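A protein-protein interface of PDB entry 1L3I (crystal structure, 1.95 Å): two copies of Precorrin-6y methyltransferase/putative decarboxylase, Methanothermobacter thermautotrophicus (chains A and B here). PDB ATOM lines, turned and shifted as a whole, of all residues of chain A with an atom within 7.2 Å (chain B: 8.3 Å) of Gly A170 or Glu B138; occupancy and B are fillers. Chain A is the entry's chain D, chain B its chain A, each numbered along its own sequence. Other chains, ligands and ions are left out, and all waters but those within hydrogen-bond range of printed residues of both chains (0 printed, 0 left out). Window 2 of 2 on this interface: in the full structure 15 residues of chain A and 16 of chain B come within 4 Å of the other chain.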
ATOM      1  N   ARG A 165      25.354  18.288 -18.675  1.00  0.00           N
ATOM      2  CA  ARG A 165      25.427  18.344 -20.136  1.00  0.00           C
ATOM      3  C   ARG A 165      24.789  19.683 -20.540  1.00  0.00           C
ATOM      4  O   ARG A 165      23.818  20.116 -19.912  1.00  0.00           O
ATOM      5  CB  ARG A 165      24.633  17.161 -20.724  1.00  0.00           C
ATOM      6  CG  ARG A 165      24.515  17.092 -22.254  1.00  0.00           C
ATOM      7  CD  ARG A 165      23.201  16.421 -22.696  1.00  0.00           C
ATOM      8  NE  ARG A 165      23.308  14.970 -22.932  1.00  0.00           N
ATOM      9  CZ  ARG A 165      22.267  14.133 -22.956  1.00  0.00           C
ATOM     10  NH1 ARG A 165      21.040  14.594 -22.752  1.00  0.00           N
ATOM     11  NH2 ARG A 165      22.431  12.854 -23.251  1.00  0.00           N
ATOM     12  N   ALA A 166      25.359  20.351 -21.543  1.00  0.00           N
ATOM     13  CA  ALA A 166      24.819  21.622 -22.035  1.00  0.00           C
ATOM     14  C   ALA A 166      23.488  21.366 -22.757  1.00  0.00           C
ATOM     15  O   ALA A 166      23.359  20.421 -23.550  1.00  0.00           O
ATOM     16  CB  ALA A 166      25.807  22.272 -22.983  1.00  0.00           C
ATOM     17  N   LEU A 167      22.489  22.183 -22.446  1.00  0.00           N
ATOM     18  CA  LEU A 167      21.161  22.067 -23.051  1.00  0.00           C
ATOM     19  C   LEU A 167      20.391  23.359 -22.800  1.00  0.00           C
ATOM     20  O   LEU A 167      20.135  23.701 -21.639  1.00  0.00           O
ATOM     21  CB  LEU A 167      20.373  20.906 -22.433  1.00  0.00           C
ATOM     22  CG  LEU A 167      18.858  20.945 -22.734  1.00  0.00           C
ATOM     23  CD1 LEU A 167      18.607  20.400 -24.151  1.00  0.00           C
ATOM     24  CD2 LEU A 167      18.043  20.179 -21.678  1.00  0.00           C
ATOM     25  N   ASP A 168      20.022  24.063 -23.876  1.00  0.00           N
ATOM     26  CA  ASP A 168      19.261  25.329 -23.784  1.00  0.00           C
ATOM     27  C   ASP A 168      20.056  26.449 -23.108  1.00  0.00           C
ATOM     28  O   ASP A 168      19.509  27.211 -22.300  1.00  0.00           O
ATOM     29  CB  ASP A 168      17.935  25.139 -22.995  1.00  0.00           C
ATOM     30  CG  ASP A 168      16.982  24.095 -23.610  1.00  0.00           C
ATOM     31  OD1 ASP A 168      17.237  23.581 -24.733  1.00  0.00           O
ATOM     32  OD2 ASP A 168      15.954  23.792 -22.940  1.00  0.00           O
ATOM     33  N   ARG A 169      21.349  26.532 -23.411  1.00  0.00           N
ATOM     34  CA  ARG A 169      22.174  27.562 -22.784  1.00  0.00           C
ATOM     35  C   ARG A 169      22.242  27.329 -21.232  1.00  0.00           C
ATOM     36  O   ARG A 169      22.778  28.155 -20.490  1.00  0.00           O
ATOM     37  CB  ARG A 169      21.573  28.942 -23.158  1.00  0.00           C
ATOM     38  CG  ARG A 169      22.133  30.174 -22.438  1.00  0.00           C
ATOM     39  CD  ARG A 169      21.164  31.350 -22.616  1.00  0.00           C
ATOM     40  NE  ARG A 169      19.763  30.923 -22.456  1.00  0.00           N
ATOM     41  CZ  ARG A 169      18.709  31.737 -22.398  1.00  0.00           C
ATOM     42  NH1 ARG A 169      18.855  33.061 -22.470  1.00  0.00           N
ATOM     43  NH2 ARG A 169      17.487  31.207 -22.316  1.00  0.00           N
ATOM     44  N   GLY A 170      21.743  26.173 -20.783  1.00  0.00           N
ATOM     45  CA  GLY A 170      21.759  25.801 -19.378  1.00  0.00           C
ATOM     46  C   GLY A 170      22.472  24.458 -19.188  1.00  0.00           C
ATOM     47  O   GLY A 170      22.963  23.877 -20.163  1.00  0.00           O
ATOM     48  N   THR A 171      22.522  23.947 -17.954  1.00  0.00           N
ATOM     49  CA  THR A 171      23.195  22.676 -17.664  1.00  0.00           C
ATOM     50  C   THR A 171      22.260  21.597 -17.155  1.00  0.00           C
ATOM     51  O   THR A 171      21.811  21.665 -16.011  1.00  0.00           O
ATOM     52  CB  THR A 171      24.295  22.860 -16.601  1.00  0.00           C
ATOM     53  OG1 THR A 171      25.113  23.980 -16.961  1.00  0.00           O
ATOM     54  CG2 THR A 171      25.171  21.595 -16.479  1.00  0.00           C
ATOM     55  N   MET A 172      21.986  20.591 -17.974  1.00  0.00           N
ATOM     56  CA  MET A 172      21.108  19.515 -17.544  1.00  0.00           C
ATOM     57  C   MET A 172      21.894  18.374 -16.922  1.00  0.00           C
ATOM     58  O   MET A 172      23.041  18.119 -17.309  1.00  0.00           O
ATOM     59  CB  MET A 172      20.237  19.025 -18.687  1.00  0.00           C
ATOM     60  CG  MET A 172      20.765  17.891 -19.499  1.00  0.00           C
ATOM     61  SD  MET A 172      19.202  17.038 -20.436  1.00  0.00           S
ATOM     62  CE  MET A 172      18.003  16.975 -18.869  1.00  0.00           C
ATOM     63  N   SER B 109      10.192  27.133 -18.794  1.00  0.00           N
ATOM     64  CA  SER B 109      10.218  28.595 -18.704  1.00  0.00           C
ATOM     65  C   SER B 109      10.869  29.305 -19.911  1.00  0.00           C
ATOM     66  O   SER B 109      10.620  30.488 -20.154  1.00  0.00           O
ATOM     67  CB  SER B 109      10.881  29.011 -17.393  1.00  0.00           C
ATOM     68  OG  SER B 109      12.187  28.464 -17.292  1.00  0.00           O
ATOM     69  N   LEU B 113      11.700  32.475 -16.772  1.00  0.00           N
ATOM     70  CA  LEU B 113      11.238  31.971 -15.479  1.00  0.00           C
ATOM     71  C   LEU B 113      10.842  33.062 -14.490  1.00  0.00           C
ATOM     72  O   LEU B 113       9.737  33.056 -13.931  1.00  0.00           O
ATOM     73  CB  LEU B 113      12.286  31.057 -14.837  1.00  0.00           C
ATOM     74  CG  LEU B 113      11.847  30.486 -13.493  1.00  0.00           C
ATOM     75  CD1 LEU B 113      10.649  29.553 -13.658  1.00  0.00           C
ATOM     76  CD2 LEU B 113      13.015  29.777 -12.848  1.00  0.00           C
ATOM     77  N   ALA B 134      12.255  21.440 -12.449  1.00  0.00           N
ATOM     78  CA  ALA B 134      13.563  21.837 -12.960  1.00  0.00           C
ATOM     79  C   ALA B 134      14.535  20.725 -13.325  1.00  0.00           C
ATOM     80  O   ALA B 134      14.841  19.868 -12.501  1.00  0.00           O
ATOM     81  CB  ALA B 134      14.224  22.765 -11.973  1.00  0.00           C
ATOM     82  N   ILE B 135      14.998  20.727 -14.570  1.00  0.00           N
ATOM     83  CA  ILE B 135      16.000  19.749 -15.007  1.00  0.00           C
ATOM     84  C   ILE B 135      17.350  20.451 -15.203  1.00  0.00           C
ATOM     85  O   ILE B 135      18.398  19.805 -15.201  1.00  0.00           O
ATOM     86  CB  ILE B 135      15.597  19.006 -16.293  1.00  0.00           C
ATOM     87  CG1 ILE B 135      15.361  19.992 -17.434  1.00  0.00           C
ATOM     88  CG2 ILE B 135      14.377  18.142 -16.037  1.00  0.00           C
ATOM     89  CD1 ILE B 135      15.111  19.308 -18.745  1.00  0.00           C
ATOM     90  N   LEU B 136      17.320  21.774 -15.385  1.00  0.00           N
ATOM     91  CA  LEU B 136      18.541  22.555 -15.535  1.00  0.00           C
ATOM     92  C   LEU B 136      18.998  23.042 -14.167  1.00  0.00           C
ATOM     93  O   LEU B 136      18.208  23.543 -13.377  1.00  0.00           O
ATOM     94  CB  LEU B 136      18.322  23.770 -16.429  1.00  0.00           C
ATOM     95  CG  LEU B 136      17.929  23.519 -17.889  1.00  0.00           C
ATOM     96  CD1 LEU B 136      17.865  24.846 -18.614  1.00  0.00           C
ATOM     97  CD2 LEU B 136      18.915  22.585 -18.552  1.00  0.00           C
ATOM     98  N   LEU B 137      20.289  22.917 -13.911  1.00  0.00           N
ATOM     99  CA  LEU B 137      20.869  23.353 -12.650  1.00  0.00           C
ATOM    100  C   LEU B 137      20.541  24.837 -12.365  1.00  0.00           C
ATOM    101  O   LEU B 137      20.212  25.210 -11.239  1.00  0.00           O
ATOM    102  CB  LEU B 137      22.393  23.141 -12.693  1.00  0.00           C
ATOM    103  CG  LEU B 137      23.303  23.839 -11.679  1.00  0.00           C
ATOM    104  CD1 LEU B 137      22.953  23.460 -10.233  1.00  0.00           C
ATOM    105  CD2 LEU B 137      24.735  23.480 -12.001  1.00  0.00           C
ATOM    106  N   GLU B 138      20.580  25.653 -13.407  1.00  0.00           N
ATOM    107  CA  GLU B 138      20.324  27.074 -13.287  1.00  0.00           C
ATOM    108  C   GLU B 138      18.899  27.338 -12.845  1.00  0.00           C
ATOM    109  O   GLU B 138      18.653  28.178 -11.977  1.00  0.00           O
ATOM    110  CB  GLU B 138      20.598  27.778 -14.605  1.00  0.00           C
ATOM    111  CG  GLU B 138      22.051  27.676 -15.086  1.00  0.00           C
ATOM    112  CD  GLU B 138      22.395  26.333 -15.732  1.00  0.00           C
ATOM    113  OE1 GLU B 138      21.498  25.507 -15.980  1.00  0.00           O
ATOM    114  OE2 GLU B 138      23.583  26.111 -16.015  1.00  0.00           O
ATOM    115  N   THR B 139      17.969  26.581 -13.409  1.00  0.00           N
ATOM    116  CA  THR B 139      16.567  26.720 -13.070  1.00  0.00           C
ATOM    117  C   THR B 139      16.311  26.406 -11.588  1.00  0.00           C
ATOM    118  O   THR B 139      15.485  27.048 -10.969  1.00  0.00           O
ATOM    119  CB  THR B 139      15.712  25.793 -13.943  1.00  0.00           C
ATOM    120  OG1 THR B 139      16.082  25.982 -15.317  1.00  0.00           O
ATOM    121  CG2 THR B 139      14.241  26.077 -13.769  1.00  0.00           C
ATOM    122  N   LYS B 140      17.030  25.431 -11.033  1.00  0.00           N
ATOM    123  CA  LYS B 140      16.838  25.061  -9.625  1.00  0.00           C
ATOM    124  C   LYS B 140      17.208  26.239  -8.735  1.00  0.00           C
ATOM    125  O   LYS B 140      16.484  26.582  -7.801  1.00  0.00           O
ATOM    126  CB  LYS B 140      17.685  23.828  -9.254  1.00  0.00           C
ATOM    127  CG  LYS B 140      17.230  22.545  -9.910  1.00  0.00           C
ATOM    128  CD  LYS B 140      18.241  21.423  -9.725  1.00  0.00           C
ATOM    129  CE  LYS B 140      17.992  20.316 -10.756  1.00  0.00           C
ATOM    130  NZ  LYS B 140      19.075  19.302 -10.779  1.00  0.00           N
ATOM    131  N   PHE B 141      18.336  26.868  -9.044  1.00  0.00           N
ATOM    132  CA  PHE B 141      18.810  28.012  -8.290  1.00  0.00           C
ATOM    133  C   PHE B 141      17.858  29.188  -8.499  1.00  0.00           C
ATOM    134  O   PHE B 141      17.383  29.796  -7.540  1.00  0.00           O
ATOM    135  CB  PHE B 141      20.202  28.403  -8.770  1.00  0.00           C
ATOM    136  CG  PHE B 141      20.761  29.611  -8.076  1.00  0.00           C
ATOM    137  CD1 PHE B 141      21.370  29.491  -6.824  1.00  0.00           C
ATOM    138  CD2 PHE B 141      20.679  30.877  -8.672  1.00  0.00           C
ATOM    139  CE1 PHE B 141      21.887  30.607  -6.176  1.00  0.00           C
ATOM    140  CE2 PHE B 141      21.195  32.005  -8.031  1.00  0.00           C
ATOM    141  CZ  PHE B 141      21.801  31.874  -6.783  1.00  0.00           C
ATOM    142  N   GLU B 142      17.574  29.492  -9.761  1.00  0.00           N
ATOM    143  CA  GLU B 142      16.692  30.594 -10.145  1.00  0.00           C
ATOM    144  C   GLU B 142      15.305  30.531  -9.502  1.00  0.00           C
ATOM    145  O   GLU B 142      14.858  31.522  -8.937  1.00  0.00           O
ATOM    146  CB  GLU B 142      16.579  30.671 -11.678  1.00  0.00           C
ATOM    147  CG  GLU B 142      16.066  32.005 -12.186  1.00  0.00           C
ATOM    148  CD  GLU B 142      16.941  33.175 -11.712  1.00  0.00           C
ATOM    149  OE1 GLU B 142      18.178  32.991 -11.550  1.00  0.00           O
ATOM    150  OE2 GLU B 142      16.382  34.280 -11.497  1.00  0.00           O
ATOM    151  N   ALA B 143      14.662  29.362  -9.552  1.00  0.00           N
ATOM    152  CA  ALA B 143      13.331  29.165  -8.981  1.00  0.00           C
ATOM    153  C   ALA B 143      13.339  29.511  -7.491  1.00  0.00           C
ATOM    154  O   ALA B 143      12.450  30.198  -6.997  1.00  0.00           O
ATOM    155  CB  ALA B 143      12.867  27.699  -9.203  1.00  0.00           C
ATOM    156  N   MET B 144      14.375  29.063  -6.798  1.00  0.00           N
ATOM    157  CA  MET B 144      14.532  29.305  -5.371  1.00  0.00           C
ATOM    158  C   MET B 144      14.677  30.793  -5.055  1.00  0.00           C
ATOM    159  O   MET B 144      13.868  31.340  -4.314  1.00  0.00           O
ATOM    160  CB  MET B 144      15.750  28.555  -4.867  1.00  0.00           C
ATOM    161  CG  MET B 144      15.625  27.059  -5.011  1.00  0.00           C
ATOM    162  SD  MET B 144      15.010  26.295  -3.398  1.00  0.00           S
ATOM    163  CE  MET B 144      16.757  26.083  -2.610  1.00  0.00           C
ATOM    164  N   GLU B 145      15.698  31.433  -5.625  1.00  0.00           N
ATOM    165  CA  GLU B 145      15.938  32.860  -5.402  1.00  0.00           C
ATOM    166  C   GLU B 145      14.675  33.661  -5.731  1.00  0.00           C
ATOM    167  O   GLU B 145      14.148  34.375  -4.887  1.00  0.00           O
ATOM    168  CB  GLU B 145      17.138  33.365  -6.243  1.00  0.00           C
ATOM    169  CG  GLU B 145      17.500  34.865  -6.005  1.00  0.00           C
ATOM    170  CD  GLU B 145      18.850  35.301  -6.605  1.00  0.00           C
ATOM    171  OE1 GLU B 145      19.005  35.262  -7.854  1.00  0.00           O
ATOM    172  OE2 GLU B 145      19.749  35.711  -5.822  1.00  0.00           O
ATOM    173  N   ILE B 182      10.641  22.494  -7.223  1.00  0.00           N
ATOM    174  CA  ILE B 182      10.749  23.653  -6.349  1.00  0.00           C
ATOM    175  C   ILE B 182       9.299  24.097  -6.109  1.00  0.00           C
ATOM    176  O   ILE B 182       8.587  24.451  -7.053  1.00  0.00           O
ATOM    177  CB  ILE B 182      11.604  24.782  -6.996  1.00  0.00           C
ATOM    178  CG1 ILE B 182      13.041  24.310  -7.193  1.00  0.00           C
ATOM    179  CG2 ILE B 182      11.590  26.036  -6.124  1.00  0.00           C
ATOM    180  CD1 ILE B 182      13.257  23.476  -8.410  1.00  0.00           C
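Among the printed residues, merely in contact across the chains: Leu A167 with Leu B136 (3.5 Å), Gly A170 with Glu B138 (3.4 Å), Thr A171 with Ile B135 (3.97 Å), Thr A171 with Leu B136 (3.4 Å), Met A172 with Ile B135 (3.6 Å) and Met A172 with Leu B136 (3.7 Å).
No position is printed for both chains. Of the 8 pairs that touch across the chains among the printed residues, none has its exchanged pair printed and touching as well.
The backbone carbonyl oxygen of Thr A171 lies within hydrogen-bond range of the backbone NH of Leu B137. N of Thr A171 lies within hydrogen-bond range of OE1 of Glu B138, at 2.7 Å.
The backbone carbonyl oxygen (O) of Met A172 lies within hydrogen-bond range of the backbone NH (N) of Arg A165 (2.7 Å).
Printed residues of chain A that touch a printed residue of chain B: Leu A167, Gly A170, Thr A171 and Met A172. Hydrophobic or aromatic side chains of chain A that line the printed part of chain B: Met A172. Among the printed residues, 8 pairs touch across the chains.
Gly A170 touches one residue of chain B. Printed residues of chain B within 4 Å of Thr A171: Ile B135 (3.97 Å), Leu B136 (3.4 Å), Leu B137 (2.9 Å) and Glu B138 (2.7 Å). Of the printed residues of chain A, Leu B137 touches Thr A171. Of chain A, only Gly A170 (3.4 Å) and Thr A171 (2.7 Å) come within 4 Å of Glu B138. Lys B140 touches none of the printed residues of chain A. Met B144 touches none of the printed residues of chain A. The nearest residue of chain B that does not touch Gly A170 is Leu B136 (4.1 Å).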
